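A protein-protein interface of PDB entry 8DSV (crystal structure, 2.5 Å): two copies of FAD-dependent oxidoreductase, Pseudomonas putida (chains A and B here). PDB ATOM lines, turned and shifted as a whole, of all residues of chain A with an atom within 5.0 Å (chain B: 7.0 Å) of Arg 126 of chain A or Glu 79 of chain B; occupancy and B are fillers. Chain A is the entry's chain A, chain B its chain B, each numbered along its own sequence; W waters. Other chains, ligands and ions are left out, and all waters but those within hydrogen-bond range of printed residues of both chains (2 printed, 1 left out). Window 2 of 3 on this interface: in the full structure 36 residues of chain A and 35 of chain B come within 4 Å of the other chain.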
ATOM      1  N   PHE A 124      23.308 -24.781  13.753  1.00  0.00           N
ATOM      2  CA  PHE A 124      24.028 -24.982  12.496  1.00  0.00           C
ATOM      3  C   PHE A 124      23.183 -25.779  11.509  1.00  0.00           C
ATOM      4  O   PHE A 124      23.526 -26.913  11.149  1.00  0.00           O
ATOM      5  CB  PHE A 124      25.356 -25.690  12.757  1.00  0.00           C
ATOM      6  CG  PHE A 124      26.347 -24.855  13.504  1.00  0.00           C
ATOM      7  CD1 PHE A 124      26.990 -23.802  12.881  1.00  0.00           C
ATOM      8  CD2 PHE A 124      26.636 -25.124  14.829  1.00  0.00           C
ATOM      9  CE1 PHE A 124      27.906 -23.032  13.566  1.00  0.00           C
ATOM     10  CE2 PHE A 124      27.549 -24.359  15.519  1.00  0.00           C
ATOM     11  CZ  PHE A 124      28.188 -23.311  14.888  1.00  0.00           C
ATOM     12  N   PRO A 125      22.075 -25.207  11.029  1.00  0.00           N
ATOM     13  CA  PRO A 125      21.347 -25.854   9.924  1.00  0.00           C
ATOM     14  C   PRO A 125      22.160 -25.922   8.651  1.00  0.00           C
ATOM     15  O   PRO A 125      21.839 -26.722   7.764  1.00  0.00           O
ATOM     16  CB  PRO A 125      20.105 -24.971   9.754  1.00  0.00           C
ATOM     17  CG  PRO A 125      20.517 -23.638  10.297  1.00  0.00           C
ATOM     18  CD  PRO A 125      21.429 -23.953  11.451  1.00  0.00           C
ATOM     19  N   ARG A 126      23.194 -25.092   8.527  1.00  0.00           N
ATOM     20  CA  ARG A 126      24.101 -25.090   7.382  1.00  0.00           C
ATOM     21  C   ARG A 126      25.521 -25.130   7.919  1.00  0.00           C
ATOM     22  O   ARG A 126      26.180 -24.086   8.034  1.00  0.00           O
ATOM     23  CB  ARG A 126      23.894 -23.856   6.508  1.00  0.00           C
ATOM     24  CG  ARG A 126      22.481 -23.647   6.030  1.00  0.00           C
ATOM     25  CD  ARG A 126      22.461 -22.589   4.963  1.00  0.00           C
ATOM     26  NE  ARG A 126      21.139 -22.011   4.778  1.00  0.00           N
ATOM     27  CZ  ARG A 126      20.835 -21.149   3.820  1.00  0.00           C
ATOM     28  NH1 ARG A 126      21.741 -20.740   2.948  1.00  0.00           N
ATOM     29  NH2 ARG A 126      19.590 -20.692   3.730  1.00  0.00           N
ATOM     30  N   PRO A 127      26.033 -26.316   8.257  1.00  0.00           N
ATOM     31  CA  PRO A 127      27.361 -26.383   8.890  1.00  0.00           C
ATOM     32  C   PRO A 127      28.458 -25.735   8.063  1.00  0.00           C
ATOM     33  O   PRO A 127      29.456 -25.283   8.637  1.00  0.00           O
ATOM     34  CB  PRO A 127      27.605 -27.890   9.059  1.00  0.00           C
ATOM     35  CG  PRO A 127      26.262 -28.529   8.989  1.00  0.00           C
ATOM     36  CD  PRO A 127      25.358 -27.626   8.205  1.00  0.00           C
ATOM     37  N   HIS A 128      28.296 -25.641   6.746  1.00  0.00           N
ATOM     38  CA  HIS A 128      29.290 -25.004   5.892  1.00  0.00           C
ATOM     39  C   HIS A 128      29.062 -23.503   5.738  1.00  0.00           C
ATOM     40  O   HIS A 128      29.758 -22.865   4.944  1.00  0.00           O
ATOM     41  CB  HIS A 128      29.313 -25.688   4.520  1.00  0.00           C
ATOM     42  CG  HIS A 128      29.750 -27.120   4.577  1.00  0.00           C
ATOM     43  ND1 HIS A 128      31.044 -27.515   4.309  1.00  0.00           N
ATOM     44  CD2 HIS A 128      29.070 -28.247   4.896  1.00  0.00           C
ATOM     45  CE1 HIS A 128      31.138 -28.826   4.450  1.00  0.00           C
ATOM     46  NE2 HIS A 128      29.955 -29.294   4.806  1.00  0.00           N
ATOM     47  N   GLU A 129      28.091 -22.940   6.456  1.00  0.00           N
ATOM     48  CA  GLU A 129      27.963 -21.497   6.659  1.00  0.00           C
ATOM     49  C   GLU A 129      27.857 -21.263   8.160  1.00  0.00           C
ATOM     50  O   GLU A 129      26.766 -21.000   8.685  1.00  0.00           O
ATOM     51  CB  GLU A 129      26.747 -20.921   5.936  1.00  0.00           C
ATOM     52  CG  GLU A 129      26.837 -20.923   4.427  1.00  0.00           C
ATOM     53  CD  GLU A 129      25.557 -20.420   3.784  1.00  0.00           C
ATOM     54  OE1 GLU A 129      25.215 -19.235   3.997  1.00  0.00           O
ATOM     55  OE2 GLU A 129      24.892 -21.208   3.071  1.00  0.00           O
ATOM     56  N   PRO A 130      28.973 -21.361   8.888  1.00  0.00           N
ATOM     57  CA  PRO A 130      28.882 -21.346  10.360  1.00  0.00           C
ATOM     58  C   PRO A 130      28.179 -20.120  10.920  1.00  0.00           C
ATOM     59  O   PRO A 130      27.534 -20.219  11.971  1.00  0.00           O
ATOM     60  CB  PRO A 130      30.351 -21.404  10.801  1.00  0.00           C
ATOM     61  CG  PRO A 130      31.070 -22.037   9.655  1.00  0.00           C
ATOM     62  CD  PRO A 130      30.352 -21.583   8.420  1.00  0.00           C
ATOM     63  N   PHE A 132      25.578 -18.573   9.714  1.00  0.00           N
ATOM     64  CA  PHE A 132      24.248 -18.388   9.142  1.00  0.00           C
ATOM     65  C   PHE A 132      23.253 -17.881  10.182  1.00  0.00           C
ATOM     66  O   PHE A 132      22.441 -16.997   9.893  1.00  0.00           O
ATOM     67  CB  PHE A 132      23.750 -19.689   8.514  1.00  0.00           C
ATOM     68  CG  PHE A 132      22.419 -19.549   7.824  1.00  0.00           C
ATOM     69  CD1 PHE A 132      22.296 -18.778   6.677  1.00  0.00           C
ATOM     70  CD2 PHE A 132      21.289 -20.170   8.330  1.00  0.00           C
ATOM     71  CE1 PHE A 132      21.073 -18.639   6.043  1.00  0.00           C
ATOM     72  CE2 PHE A 132      20.064 -20.033   7.702  1.00  0.00           C
ATOM     73  CZ  PHE A 132      19.956 -19.267   6.558  1.00  0.00           C
ATOM     74  N   TRP B  58      17.593 -30.412  -6.336  1.00  0.00           N
ATOM     75  CA  TRP B  58      17.975 -30.285  -4.938  1.00  0.00           C
ATOM     76  C   TRP B  58      19.269 -31.037  -4.656  1.00  0.00           C
ATOM     77  O   TRP B  58      19.479 -32.142  -5.165  1.00  0.00           O
ATOM     78  CB  TRP B  58      16.855 -30.785  -4.023  1.00  0.00           C
ATOM     79  CG  TRP B  58      15.615 -29.940  -4.107  1.00  0.00           C
ATOM     80  CD1 TRP B  58      15.486 -28.637  -3.723  1.00  0.00           C
ATOM     81  CD2 TRP B  58      14.333 -30.339  -4.606  1.00  0.00           C
ATOM     82  NE1 TRP B  58      14.203 -28.201  -3.949  1.00  0.00           N
ATOM     83  CE2 TRP B  58      13.474 -29.228  -4.488  1.00  0.00           C
ATOM     84  CE3 TRP B  58      13.824 -31.530  -5.127  1.00  0.00           C
ATOM     85  CZ2 TRP B  58      12.136 -29.273  -4.879  1.00  0.00           C
ATOM     86  CZ3 TRP B  58      12.498 -31.575  -5.515  1.00  0.00           C
ATOM     87  CH2 TRP B  58      11.668 -30.452  -5.389  1.00  0.00           C
ATOM     88  N   TRP B  61      25.202 -30.914   1.189  1.00  0.00           N
ATOM     89  CA  TRP B  61      26.624 -31.057   1.492  1.00  0.00           C
ATOM     90  C   TRP B  61      26.999 -32.469   1.937  1.00  0.00           C
ATOM     91  O   TRP B  61      28.185 -32.814   1.920  1.00  0.00           O
ATOM     92  CB  TRP B  61      27.057 -30.049   2.563  1.00  0.00           C
ATOM     93  CG  TRP B  61      26.132 -29.953   3.736  1.00  0.00           C
ATOM     94  CD1 TRP B  61      26.195 -30.674   4.895  1.00  0.00           C
ATOM     95  CD2 TRP B  61      25.001 -29.087   3.863  1.00  0.00           C
ATOM     96  NE1 TRP B  61      25.170 -30.312   5.732  1.00  0.00           N
ATOM     97  CE2 TRP B  61      24.423 -29.338   5.122  1.00  0.00           C
ATOM     98  CE3 TRP B  61      24.418 -28.128   3.031  1.00  0.00           C
ATOM     99  CZ2 TRP B  61      23.293 -28.660   5.571  1.00  0.00           C
ATOM    100  CZ3 TRP B  61      23.293 -27.456   3.477  1.00  0.00           C
ATOM    101  CH2 TRP B  61      22.742 -27.726   4.737  1.00  0.00           C
ATOM    102  N   GLY B  76      26.692 -21.274  -3.964  1.00  0.00           N
ATOM    103  CA  GLY B  76      26.023 -21.514  -2.703  1.00  0.00           C
ATOM    104  C   GLY B  76      24.732 -22.290  -2.895  1.00  0.00           C
ATOM    105  O   GLY B  76      24.502 -22.925  -3.927  1.00  0.00           O
ATOM    106  N   VAL B  77      23.874 -22.228  -1.880  1.00  0.00           N
ATOM    107  CA  VAL B  77      22.592 -22.920  -1.900  1.00  0.00           C
ATOM    108  C   VAL B  77      21.459 -21.902  -1.925  1.00  0.00           C
ATOM    109  O   VAL B  77      21.629 -20.723  -1.605  1.00  0.00           O
ATOM    110  CB  VAL B  77      22.424 -23.876  -0.697  1.00  0.00           C
ATOM    111  CG1 VAL B  77      23.371 -25.049  -0.809  1.00  0.00           C
ATOM    112  CG2 VAL B  77      22.637 -23.133   0.627  1.00  0.00           C
ATOM    113  N   VAL B  78      20.285 -22.381  -2.325  1.00  0.00           N
ATOM    114  CA  VAL B  78      19.041 -21.619  -2.317  1.00  0.00           C
ATOM    115  C   VAL B  78      18.020 -22.445  -1.544  1.00  0.00           C
ATOM    116  O   VAL B  78      17.734 -23.588  -1.916  1.00  0.00           O
ATOM    117  CB  VAL B  78      18.541 -21.318  -3.739  1.00  0.00           C
ATOM    118  CG1 VAL B  78      17.269 -20.488  -3.697  1.00  0.00           C
ATOM    119  CG2 VAL B  78      19.627 -20.600  -4.547  1.00  0.00           C
ATOM    120  N   GLU B  79      17.485 -21.882  -0.468  1.00  0.00           N
ATOM    121  CA  GLU B  79      16.621 -22.634   0.426  1.00  0.00           C
ATOM    122  C   GLU B  79      15.175 -22.555  -0.044  1.00  0.00           C
ATOM    123  O   GLU B  79      14.645 -21.463  -0.268  1.00  0.00           O
ATOM    124  CB  GLU B  79      16.741 -22.120   1.861  1.00  0.00           C
ATOM    125  CG  GLU B  79      16.203 -23.101   2.894  1.00  0.00           C
ATOM    126  CD  GLU B  79      16.219 -22.550   4.305  1.00  0.00           C
ATOM    127  OE1 GLU B  79      17.157 -21.801   4.646  1.00  0.00           O
ATOM    128  OE2 GLU B  79      15.288 -22.862   5.075  1.00  0.00           O
ATOM    129  N   ASP B  80      14.543 -23.704  -0.167  1.00  0.00           N
ATOM    130  CA  ASP B  80      13.111 -23.727  -0.402  1.00  0.00           C
ATOM    131  C   ASP B  80      12.359 -23.797   0.925  1.00  0.00           C
ATOM    132  O   ASP B  80      12.891 -24.297   1.922  1.00  0.00           O
ATOM    133  CB  ASP B  80      12.737 -24.923  -1.276  1.00  0.00           C
ATOM    134  CG  ASP B  80      13.006 -24.671  -2.749  1.00  0.00           C
ATOM    135  OD1 ASP B  80      13.127 -23.492  -3.136  1.00  0.00           O
ATOM    136  OD2 ASP B  80      13.108 -25.648  -3.519  1.00  0.00           O
ATOM    137  N   PRO B  81      11.143 -23.241   0.980  1.00  0.00           N
ATOM    138  CA  PRO B  81      10.472 -23.075   2.276  1.00  0.00           C
ATOM    139  C   PRO B  81       9.915 -24.377   2.829  1.00  0.00           C
ATOM    140  O   PRO B  81       8.700 -24.600   2.810  1.00  0.00           O
ATOM    141  CB  PRO B  81       9.360 -22.064   1.962  1.00  0.00           C
ATOM    142  CG  PRO B  81       9.044 -22.307   0.532  1.00  0.00           C
ATOM    143  CD  PRO B  81      10.343 -22.687  -0.127  1.00  0.00           C
ATOM    144  N   LEU B  82      10.798 -25.243   3.324  1.00  0.00           N
ATOM    145  CA  LEU B  82      10.399 -26.511   3.921  1.00  0.00           C
ATOM    146  C   LEU B  82      10.264 -26.445   5.434  1.00  0.00           C
ATOM    147  O   LEU B  82       9.455 -27.185   6.002  1.00  0.00           O
ATOM    148  CB  LEU B  82      11.399 -27.612   3.557  1.00  0.00           C
ATOM    149  CG  LEU B  82      11.218 -28.290   2.195  1.00  0.00           C
ATOM    150  CD1 LEU B  82       9.933 -29.122   2.144  1.00  0.00           C
ATOM    151  CD2 LEU B  82      11.234 -27.260   1.077  1.00  0.00           C
ATOM    152  N   THR B  83      11.069 -25.624   6.103  1.00  0.00           N
ATOM    153  CA  THR B  83      10.965 -25.491   7.547  1.00  0.00           C
ATOM    154  C   THR B  83       9.711 -24.712   7.930  1.00  0.00           C
ATOM    155  O   THR B  83       9.138 -23.957   7.134  1.00  0.00           O
ATOM    156  CB  THR B  83      12.199 -24.785   8.118  1.00  0.00           C
ATOM    157  OG1 THR B  83      12.259 -23.437   7.630  1.00  0.00           O
ATOM    158  CG2 THR B  83      13.474 -25.524   7.723  1.00  0.00           C
ATOM    159  N   HIS B 201      15.320 -29.704  -0.100  1.00  0.00           N
ATOM    160  CA  HIS B 201      15.474 -28.498   0.710  1.00  0.00           C
ATOM    161  C   HIS B 201      16.317 -27.424   0.038  1.00  0.00           C
ATOM    162  O   HIS B 201      15.949 -26.248   0.074  1.00  0.00           O
ATOM    163  CB  HIS B 201      16.077 -28.838   2.082  1.00  0.00           C
ATOM    164  CG  HIS B 201      15.881 -27.761   3.109  1.00  0.00           C
ATOM    165  ND1 HIS B 201      16.337 -27.875   4.406  1.00  0.00           N
ATOM    166  CD2 HIS B 201      15.282 -26.549   3.029  1.00  0.00           C
ATOM    167  CE1 HIS B 201      16.028 -26.780   5.078  1.00  0.00           C
ATOM    168  NE2 HIS B 201      15.387 -25.959   4.266  1.00  0.00           N
ATOM    169  N   TYR B 202      17.432 -27.788  -0.582  1.00  0.00           N
ATOM    170  CA  TYR B 202      18.383 -26.819  -1.103  1.00  0.00           C
ATOM    171  C   TYR B 202      18.591 -27.039  -2.592  1.00  0.00           C
ATOM    172  O   TYR B 202      18.805 -28.172  -3.033  1.00  0.00           O
ATOM    173  CB  TYR B 202      19.714 -26.917  -0.352  1.00  0.00           C
ATOM    174  CG  TYR B 202      19.588 -26.580   1.117  1.00  0.00           C
ATOM    175  CD1 TYR B 202      19.489 -25.261   1.540  1.00  0.00           C
ATOM    176  CD2 TYR B 202      19.544 -27.579   2.079  1.00  0.00           C
ATOM    177  CE1 TYR B 202      19.363 -24.947   2.883  1.00  0.00           C
ATOM    178  CE2 TYR B 202      19.419 -27.274   3.427  1.00  0.00           C
ATOM    179  CZ  TYR B 202      19.328 -25.960   3.819  1.00  0.00           C
ATOM    180  OH  TYR B 202      19.202 -25.657   5.150  1.00  0.00           O
ATOM    181  N   ARG B 203      18.519 -25.954  -3.353  1.00  0.00           N
ATOM    182  CA  ARG B 203      18.835 -25.916  -4.771  1.00  0.00           C
ATOM    183  C   ARG B 203      20.156 -25.189  -4.975  1.00  0.00           C
ATOM    184  O   ARG B 203      20.719 -24.610  -4.045  1.00  0.00           O
ATOM    185  CB  ARG B 203      17.722 -25.212  -5.553  1.00  0.00           C
ATOM    186  CG  ARG B 203      16.453 -26.029  -5.695  1.00  0.00           C
ATOM    187  CD  ARG B 203      15.442 -25.301  -6.560  1.00  0.00           C
ATOM    188  NE  ARG B 203      15.004 -24.052  -5.946  1.00  0.00           N
ATOM    189  CZ  ARG B 203      14.785 -22.918  -6.600  1.00  0.00           C
ATOM    190  NH1 ARG B 203      14.935 -22.833  -7.915  1.00  0.00           N
ATOM    191  NH2 ARG B 203      14.391 -21.844  -5.923  1.00  0.00           N
ATOM    192  N   ARG B 301       3.447 -22.199   3.528  1.00  0.00           N
ATOM    193  CA  ARG B 301       4.399 -23.292   3.396  1.00  0.00           C
ATOM    194  C   ARG B 301       3.621 -24.588   3.564  1.00  0.00           C
ATOM    195  O   ARG B 301       3.139 -24.891   4.660  1.00  0.00           O
ATOM    196  CB  ARG B 301       5.520 -23.173   4.427  1.00  0.00           C
ATOM    197  CG  ARG B 301       6.247 -21.836   4.409  1.00  0.00           C
ATOM    198  CD  ARG B 301       7.431 -21.829   5.371  1.00  0.00           C
ATOM    199  NE  ARG B 301       8.367 -20.746   5.087  1.00  0.00           N
ATOM    200  CZ  ARG B 301       9.667 -20.781   5.351  1.00  0.00           C
ATOM    201  NH1 ARG B 301      10.240 -21.850   5.880  1.00  0.00           N
ATOM    202  NH2 ARG B 301      10.415 -19.716   5.070  1.00  0.00           N
ATOM    203  N   HIS B 318       6.962 -23.924  -3.550  1.00  0.00           N
ATOM    204  CA  HIS B 318       8.118 -23.330  -4.212  1.00  0.00           C
ATOM    205  C   HIS B 318       8.292 -21.864  -3.813  1.00  0.00           C
ATOM    206  O   HIS B 318       9.409 -21.414  -3.530  1.00  0.00           O
ATOM    207  CB  HIS B 318       7.955 -23.459  -5.731  1.00  0.00           C
ATOM    208  CG  HIS B 318       9.062 -22.834  -6.520  1.00  0.00           C
ATOM    209  ND1 HIS B 318      10.239 -23.493  -6.806  1.00  0.00           N
ATOM    210  CD2 HIS B 318       9.170 -21.610  -7.091  1.00  0.00           C
ATOM    211  CE1 HIS B 318      11.024 -22.702  -7.517  1.00  0.00           C
ATOM    212  NE2 HIS B 318      10.399 -21.553  -7.703  1.00  0.00           N
HETATM  213  O   HOH W   1      19.416 -27.754   7.000  1.00  0.00           O
HETATM  214  O   HOH W   2      25.460 -21.251   0.631  1.00  0.00           O
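The side-chain carboxylate of Glu 79 of chain B is in salt-bridge range of the guanidinium group of Arg 126 of chain A (2.8 Å).
NE2 of His 201 of chain B is in hydrogen-bond range of OE2 of Glu 79 of chain B.
The guanidinium group (NH1) of Arg 126 of chain A is in salt-bridge range of the side-chain carboxylate (OE2) of Glu 129 of chain A, 3.2 Å away.
CZ2 of Trp 61 of chain B touches O of Pro 125 of chain A, 3.3 Å away.
Pro 125 of chain A touches Tyr 202 of chain B.
Arg 126 of chain A touches Trp 61 of chain B.
Val 77 of chain B touches Arg 126 of chain A (CG2 to NH1, 3.5 Å).
Tyr 202 of chain B touches Arg 126 of chain A (CE1 to NE, 3.9 Å).
Trp 61 of chain B touches Pro 127 of chain A (CZ2 to CD, 3.5 Å).
His 128 of chain A touches Trp 61 of chain B.
Val 77 of chain B touches Glu 129 of chain A.
Arg 126 of chain A touches just these residues of chain B: Trp 61, Val 77, Glu 79 and Tyr 202.
Of chain A, only Arg 126 (2.8 Å) comes within 4 Å of Glu 79 of chain B.
Of the printed residues of chain A, Trp 61 of chain B touches Pro 125, Arg 126, Pro 127 and His 128.
Of the printed residues of chain B, His 128 of chain A touches Trp 61 (3.6 Å).
Printed residues of chain A within 4 Å of Val 77 of chain B: Arg 126 and Glu 129.
Of the printed residues of chain B, Pro 127 of chain A touches Trp 61 (3.5 Å).
Printed residues of chain B within 4 Å of Glu 129 of chain A: Val 77 (3.8 Å).
His 318 of chain B touches none of the printed residues of chain A.
Arg 203 of chain B touches none of the printed residues of chain A.
Of the 8 printed residues of chain A, 5 touch a printed residue of chain B.
Printed residues of chain A that touch a printed residue of chain B: Pro 125, Arg 126, Pro 127, His 128 and Glu 129.
Hydrophobic or aromatic side chains of chain A that line the printed part of chain B: Pro 127 and His 128.
Hydrophobic or aromatic side chains of chain B within 4 Å of the printed part of chain A: Trp 61, Val 77 and Tyr 202.
Among the printed residues, 9 pairs touch across the chains.
Among the printed residues, Asp or Glu carboxylates within 4 Å of a Lys or Arg side-chain nitrogen of the other chain: Arg 126 of chain A with Glu 79 of chain B.
No position is printed for both chains.
Of the 9 pairs that touch across the chains among the printed residues, none has its exchanged pair printed and touching as well.
Water W2 lies within hydrogen-bond range of the side-chain carboxylate (OE2) of Glu 129 of chain A and the backbone NH (N) of Val 77 of chain B.
Water W1 bridges O of Pro 125 of chain A (2.7 Å) and OH of Tyr 202 of chain B (2.8 Å).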
